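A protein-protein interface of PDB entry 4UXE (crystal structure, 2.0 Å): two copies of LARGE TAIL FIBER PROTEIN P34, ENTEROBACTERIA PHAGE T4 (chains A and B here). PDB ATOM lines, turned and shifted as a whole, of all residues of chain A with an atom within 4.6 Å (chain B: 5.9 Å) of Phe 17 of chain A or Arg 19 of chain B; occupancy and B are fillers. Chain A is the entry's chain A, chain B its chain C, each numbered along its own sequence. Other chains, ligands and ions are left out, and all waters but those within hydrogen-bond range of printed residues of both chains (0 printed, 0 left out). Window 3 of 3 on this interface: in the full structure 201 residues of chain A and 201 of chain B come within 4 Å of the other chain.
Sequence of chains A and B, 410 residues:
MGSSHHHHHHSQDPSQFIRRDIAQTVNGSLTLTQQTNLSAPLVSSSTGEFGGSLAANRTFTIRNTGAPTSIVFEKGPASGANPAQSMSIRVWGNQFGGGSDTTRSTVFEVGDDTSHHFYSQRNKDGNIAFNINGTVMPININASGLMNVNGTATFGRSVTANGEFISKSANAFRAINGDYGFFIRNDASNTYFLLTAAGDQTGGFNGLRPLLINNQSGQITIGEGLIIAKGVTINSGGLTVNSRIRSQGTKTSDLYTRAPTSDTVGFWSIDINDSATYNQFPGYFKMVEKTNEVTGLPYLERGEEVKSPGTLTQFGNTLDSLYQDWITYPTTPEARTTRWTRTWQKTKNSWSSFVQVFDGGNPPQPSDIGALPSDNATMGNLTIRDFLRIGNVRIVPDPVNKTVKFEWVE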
ATOM      1  N   PRO A  14     -12.494 -20.387  22.110  1.00  0.00           N
ATOM      2  CA  PRO A  14     -12.403 -21.756  21.596  1.00  0.00           C
ATOM      3  C   PRO A  14     -13.338 -22.719  22.343  1.00  0.00           C
ATOM      4  O   PRO A  14     -14.270 -22.271  23.022  1.00  0.00           O
ATOM      5  CB  PRO A  14     -10.928 -22.123  21.840  1.00  0.00           C
ATOM      6  CG  PRO A  14     -10.422 -21.141  22.895  1.00  0.00           C
ATOM      7  CD  PRO A  14     -11.504 -20.123  23.169  1.00  0.00           C
ATOM      8  N   SER A  15     -13.100 -24.025  22.196  1.00  0.00           N
ATOM      9  CA  SER A  15     -13.794 -25.046  22.996  1.00  0.00           C
ATOM     10  C   SER A  15     -12.930 -25.524  24.182  1.00  0.00           C
ATOM     11  O   SER A  15     -12.618 -26.717  24.327  1.00  0.00           O
ATOM     12  CB  SER A  15     -14.279 -26.208  22.121  1.00  0.00           C
ATOM     13  OG  SER A  15     -15.368 -25.801  21.311  1.00  0.00           O
ATOM     14  N   GLN A  16     -12.534 -24.555  25.007  1.00  0.00           N
ATOM     15  CA  GLN A  16     -11.930 -24.818  26.300  1.00  0.00           C
ATOM     16  C   GLN A  16     -13.024 -24.636  27.354  1.00  0.00           C
ATOM     17  O   GLN A  16     -12.885 -23.872  28.316  1.00  0.00           O
ATOM     18  CB  GLN A  16     -10.731 -23.896  26.542  1.00  0.00           C
ATOM     19  CG  GLN A  16      -9.647 -24.502  27.442  1.00  0.00           C
ATOM     20  CD  GLN A  16      -9.022 -25.779  26.872  1.00  0.00           C
ATOM     21  OE1 GLN A  16      -9.678 -26.826  26.775  1.00  0.00           O
ATOM     22  NE2 GLN A  16      -7.740 -25.696  26.509  1.00  0.00           N
ATOM     23  N   PHE A  17     -14.126 -25.341  27.115  1.00  0.00           N
ATOM     24  CA  PHE A  17     -15.290 -25.383  27.989  1.00  0.00           C
ATOM     25  C   PHE A  17     -15.686 -26.846  28.174  1.00  0.00           C
ATOM     26  O   PHE A  17     -15.379 -27.693  27.324  1.00  0.00           O
ATOM     27  CB  PHE A  17     -16.453 -24.595  27.376  1.00  0.00           C
ATOM     28  CG  PHE A  17     -16.244 -23.104  27.369  1.00  0.00           C
ATOM     29  CD1 PHE A  17     -15.609 -22.477  26.299  1.00  0.00           C
ATOM     30  CD2 PHE A  17     -16.694 -22.321  28.432  1.00  0.00           C
ATOM     31  CE1 PHE A  17     -15.418 -21.092  26.292  1.00  0.00           C
ATOM     32  CE2 PHE A  17     -16.511 -20.934  28.434  1.00  0.00           C
ATOM     33  CZ  PHE A  17     -15.871 -20.321  27.364  1.00  0.00           C
ATOM     34  N   ILE A  18     -16.360 -27.147  29.281  1.00  0.00           N
ATOM     35  CA  ILE A  18     -16.713 -28.533  29.582  1.00  0.00           C
ATOM     36  C   ILE A  18     -17.976 -28.926  28.831  1.00  0.00           C
ATOM     37  O   ILE A  18     -19.020 -28.289  28.981  1.00  0.00           O
ATOM     38  CB  ILE A  18     -16.890 -28.809  31.105  1.00  0.00           C
ATOM     39  CG1 ILE A  18     -15.837 -28.073  31.941  1.00  0.00           C
ATOM     40  CG2 ILE A  18     -16.825 -30.308  31.372  1.00  0.00           C
ATOM     41  CD1 ILE A  18     -16.165 -27.986  33.424  1.00  0.00           C
ATOM     42  N   ARG A  19     -17.861 -29.971  28.014  1.00  0.00           N
ATOM     43  CA  ARG A  19     -19.007 -30.542  27.307  1.00  0.00           C
ATOM     44  C   ARG A  19     -19.973 -31.206  28.286  1.00  0.00           C
ATOM     45  O   ARG A  19     -19.559 -31.868  29.243  1.00  0.00           O
ATOM     46  CB  ARG A  19     -18.563 -31.548  26.238  1.00  0.00           C
ATOM     47  CG  ARG A  19     -17.975 -30.934  24.958  1.00  0.00           C
ATOM     48  CD  ARG A  19     -19.053 -30.496  23.955  1.00  0.00           C
ATOM     49  NE  ARG A  19     -19.986 -31.574  23.623  1.00  0.00           N
ATOM     50  CZ  ARG A  19     -19.765 -32.516  22.708  1.00  0.00           C
ATOM     51  NH1 ARG A  19     -18.633 -32.525  22.011  1.00  0.00           N
ATOM     52  NH2 ARG A  19     -20.677 -33.455  22.488  1.00  0.00           N
ATOM     53  N   GLN A  24     -15.711 -35.921  29.984  1.00  0.00           N
ATOM     54  CA  GLN A  24     -14.801 -34.769  30.031  1.00  0.00           C
ATOM     55  C   GLN A  24     -13.772 -34.836  31.159  1.00  0.00           C
ATOM     56  O   GLN A  24     -14.121 -35.127  32.297  1.00  0.00           O
ATOM     57  CB  GLN A  24     -15.600 -33.473  30.167  1.00  0.00           C
ATOM     58  CG  GLN A  24     -16.476 -33.152  28.970  1.00  0.00           C
ATOM     59  CD  GLN A  24     -15.717 -32.451  27.849  1.00  0.00           C
ATOM     60  OE1 GLN A  24     -15.491 -31.241  27.899  1.00  0.00           O
ATOM     61  NE2 GLN A  24     -15.339 -33.210  26.825  1.00  0.00           N
ATOM     62  N   VAL A  26     -11.539 -32.449  33.381  1.00  0.00           N
ATOM     63  CA  VAL A  26     -11.505 -31.044  33.771  1.00  0.00           C
ATOM     64  C   VAL A  26     -10.179 -30.731  34.462  1.00  0.00           C
ATOM     65  O   VAL A  26      -9.828 -31.366  35.457  1.00  0.00           O
ATOM     66  CB  VAL A  26     -12.699 -30.694  34.686  1.00  0.00           C
ATOM     67  CG1 VAL A  26     -12.681 -29.225  35.094  1.00  0.00           C
ATOM     68  CG2 VAL A  26     -14.008 -31.048  33.993  1.00  0.00           C
ATOM     69  N   SER B  15     -19.748 -15.245  29.537  1.00  0.00           N
ATOM     70  CA  SER B  15     -19.332 -16.649  29.591  1.00  0.00           C
ATOM     71  C   SER B  15     -20.044 -17.375  30.735  1.00  0.00           C
ATOM     72  O   SER B  15     -19.436 -17.727  31.752  1.00  0.00           O
ATOM     73  CB  SER B  15     -17.809 -16.771  29.714  1.00  0.00           C
ATOM     74  OG  SER B  15     -17.349 -16.234  30.943  1.00  0.00           O
ATOM     75  N   PHE B  17     -20.690 -20.175  30.889  1.00  0.00           N
ATOM     76  CA  PHE B  17     -20.280 -21.560  30.675  1.00  0.00           C
ATOM     77  C   PHE B  17     -18.975 -21.837  31.431  1.00  0.00           C
ATOM     78  O   PHE B  17     -18.182 -20.924  31.680  1.00  0.00           O
ATOM     79  CB  PHE B  17     -20.134 -21.865  29.178  1.00  0.00           C
ATOM     80  CG  PHE B  17     -21.418 -21.729  28.391  1.00  0.00           C
ATOM     81  CD1 PHE B  17     -21.796 -20.500  27.847  1.00  0.00           C
ATOM     82  CD2 PHE B  17     -22.243 -22.831  28.184  1.00  0.00           C
ATOM     83  CE1 PHE B  17     -22.981 -20.369  27.119  1.00  0.00           C
ATOM     84  CE2 PHE B  17     -23.431 -22.714  27.454  1.00  0.00           C
ATOM     85  CZ  PHE B  17     -23.799 -21.480  26.922  1.00  0.00           C
ATOM     86  N   ILE B  18     -18.764 -23.099  31.796  1.00  0.00           N
ATOM     87  CA  ILE B  18     -17.674 -23.467  32.696  1.00  0.00           C
ATOM     88  C   ILE B  18     -16.400 -23.823  31.943  1.00  0.00           C
ATOM     89  O   ILE B  18     -16.416 -24.672  31.050  1.00  0.00           O
ATOM     90  CB  ILE B  18     -18.071 -24.634  33.646  1.00  0.00           C
ATOM     91  CG1 ILE B  18     -19.517 -24.471  34.130  1.00  0.00           C
ATOM     92  CG2 ILE B  18     -17.100 -24.708  34.819  1.00  0.00           C
ATOM     93  CD1 ILE B  18     -20.023 -25.588  34.997  1.00  0.00           C
ATOM     94  N   ARG B  19     -15.304 -23.168  32.324  1.00  0.00           N
ATOM     95  CA  ARG B  19     -13.990 -23.418  31.734  1.00  0.00           C
ATOM     96  C   ARG B  19     -13.438 -24.787  32.120  1.00  0.00           C
ATOM     97  O   ARG B  19     -13.570 -25.231  33.265  1.00  0.00           O
ATOM     98  CB  ARG B  19     -12.994 -22.321  32.121  1.00  0.00           C
ATOM     99  CG  ARG B  19     -13.380 -20.905  31.666  1.00  0.00           C
ATOM    100  CD  ARG B  19     -13.283 -20.709  30.147  1.00  0.00           C
ATOM    101  NE  ARG B  19     -11.993 -21.144  29.613  1.00  0.00           N
ATOM    102  CZ  ARG B  19     -10.869 -20.434  29.675  1.00  0.00           C
ATOM    103  NH1 ARG B  19     -10.851 -19.238  30.252  1.00  0.00           N
ATOM    104  NH2 ARG B  19      -9.753 -20.927  29.160  1.00  0.00           N
ATOM    105  N   ARG B  20     -12.808 -25.434  31.146  1.00  0.00           N
ATOM    106  CA  ARG B  20     -12.336 -26.805  31.258  1.00  0.00           C
ATOM    107  C   ARG B  20     -10.825 -26.854  31.537  1.00  0.00           C
ATOM    108  O   ARG B  20     -10.198 -27.918  31.459  1.00  0.00           O
ATOM    109  CB  ARG B  20     -12.685 -27.544  29.962  1.00  0.00           C
ATOM    110  CG  ARG B  20     -12.518 -29.045  29.972  1.00  0.00           C
ATOM    111  CD  ARG B  20     -12.568 -29.571  28.552  1.00  0.00           C
ATOM    112  NE  ARG B  20     -11.680 -30.716  28.356  1.00  0.00           N
ATOM    113  CZ  ARG B  20     -10.374 -30.626  28.107  1.00  0.00           C
ATOM    114  NH1 ARG B  20      -9.782 -29.439  28.022  1.00  0.00           N
ATOM    115  NH2 ARG B  20      -9.654 -31.730  27.946  1.00  0.00           N
ATOM    116  N   ASP B  21     -10.240 -25.702  31.872  1.00  0.00           N
ATOM    117  CA  ASP B  21      -8.795 -25.626  32.116  1.00  0.00           C
ATOM    118  C   ASP B  21      -8.419 -24.507  33.088  1.00  0.00           C
ATOM    119  O   ASP B  21      -7.239 -24.219  33.301  1.00  0.00           O
ATOM    120  CB  ASP B  21      -8.034 -25.480  30.785  1.00  0.00           C
ATOM    121  CG  ASP B  21      -6.744 -26.299  30.745  1.00  0.00           C
ATOM    122  OD1 ASP B  21      -5.813 -26.013  31.539  1.00  0.00           O
ATOM    123  OD2 ASP B  21      -6.658 -27.224  29.903  1.00  0.00           O
ATOM    124  N   ILE B  22      -9.426 -23.894  33.697  1.00  0.00           N
ATOM    125  CA  ILE B  22      -9.197 -22.776  34.606  1.00  0.00           C
ATOM    126  C   ILE B  22     -10.084 -22.864  35.854  1.00  0.00           C
ATOM    127  O   ILE B  22     -11.175 -23.427  35.801  1.00  0.00           O
ATOM    128  CB  ILE B  22      -9.307 -21.421  33.830  1.00  0.00           C
ATOM    129  CG1 ILE B  22      -7.900 -20.936  33.455  1.00  0.00           C
ATOM    130  CG2 ILE B  22     -10.091 -20.346  34.610  1.00  0.00           C
ATOM    131  CD1 ILE B  22      -7.766 -20.460  32.017  1.00  0.00           C
ATOM    132  N   GLN B  24     -12.748 -22.228  38.384  1.00  0.00           N
ATOM    133  CA  GLN B  24     -14.101 -21.738  38.129  1.00  0.00           C
ATOM    134  C   GLN B  24     -14.974 -21.807  39.370  1.00  0.00           C
ATOM    135  O   GLN B  24     -14.743 -22.628  40.256  1.00  0.00           O
ATOM    136  CB  GLN B  24     -14.762 -22.576  37.027  1.00  0.00           C
ATOM    137  CG  GLN B  24     -14.146 -22.433  35.642  1.00  0.00           C
ATOM    138  CD  GLN B  24     -14.502 -21.115  34.969  1.00  0.00           C
ATOM    139  OE1 GLN B  24     -15.543 -20.996  34.317  1.00  0.00           O
ATOM    140  NE2 GLN B  24     -13.628 -20.128  35.110  1.00  0.00           N
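NE of Arg 19 of chain B sits at hydrogen-bond distance from O of Gln 16 of chain A, 3.1 Å away. The side-chain amide oxygen of Gln 16 of chain A sits at hydrogen-bond distance from the guanidinium group of Arg 20 of chain B, 2.9 Å away. The backbone NH (N) of Ile 18 of chain A sits at hydrogen-bond distance from the backbone carbonyl oxygen (O) of Ile 18 of chain B (3.0 Å).
Phe 17 of chain A touches just these residues of chain B: Phe 17, Ile 18, Arg 19 and Arg 20. Printed residues of chain B within 4 Å of Ile 18 of chain A: Ile 18, Arg 19 and Arg 20. Arg 19 of chain A touches none of the printed residues of chain B. Val 26 of chain A touches none of the printed residues of chain B. Of the printed residues of chain A, Arg 20 of chain B touches Gln 16 (2.9 Å), Phe 17 (3.6 Å), Ile 18 (3.8 Å) and Gln 24 (3.4 Å). The nearest residue of chain B that does not touch Phe 17 of chain A is Ser 15 of chain B (4.5 Å).
OE1 of Gln 24 of chain B sits at hydrogen-bond distance from N of Arg 19 of chain B. The backbone NH (N) of Arg 19 of chain A sits at hydrogen-bond distance from the side-chain amide oxygen (OE1) of Gln 24 of chain A, 2.7 Å away.
Among the printed residues, pairs that only touch across the chains: Phe 17 of chain A with Ile 18 of chain B (3.3 Å), Gln 24 of chain A with Arg 20 of chain B (3.4 Å), Phe 17 of chain A with Phe 17 of chain B (3.5 Å), Phe 17 of chain A with Arg 20 of chain B (3.6 Å), Phe 17 of chain A with Arg 19 of chain B (3.7 Å), Ile 18 of chain A with Arg 20 of chain B (3.8 Å), Ile 18 of chain A with Arg 19 of chain B (3.8 Å) and Gln 16 of chain A with Asp 21 of chain B (3.8 Å).
Printed residues of chain B that touch a printed residue of chain A: Phe 17, Ile 18, Arg 19, Arg 20 and Asp 21. Of the 8 printed residues of chain A, 4 touch a printed residue of chain B. Hydrophobic or aromatic side chains of chain A that line the printed part of chain B: Phe 17 and Ile 18. Among the printed residues, no Asp or Glu carboxylate lies within 4 Å of a Lys or Arg side-chain nitrogen of the other chain.
Phe 17 of chain A touches Ile 18 of chain B, but with the chains exchanged Ile 18 of chain A does not touch Phe 17 of chain B (6.3 Å). Phe 17 of chain A touches Arg 19 of chain B, but with the chains exchanged Arg 19 of chain A does not touch Phe 17 of chain B (8.4 Å). Ile 18 of chain A touches its own counterpart, Ile 18 of chain B. Ile 18 of chain A touches Arg 19 of chain B, but with the chains exchanged Arg 19 of chain A does not touch Ile 18 of chain B (6.3 Å). Of the 11 pairs that touch across the chains among the printed residues, 2 have their exchanged pair printed and touching as well.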
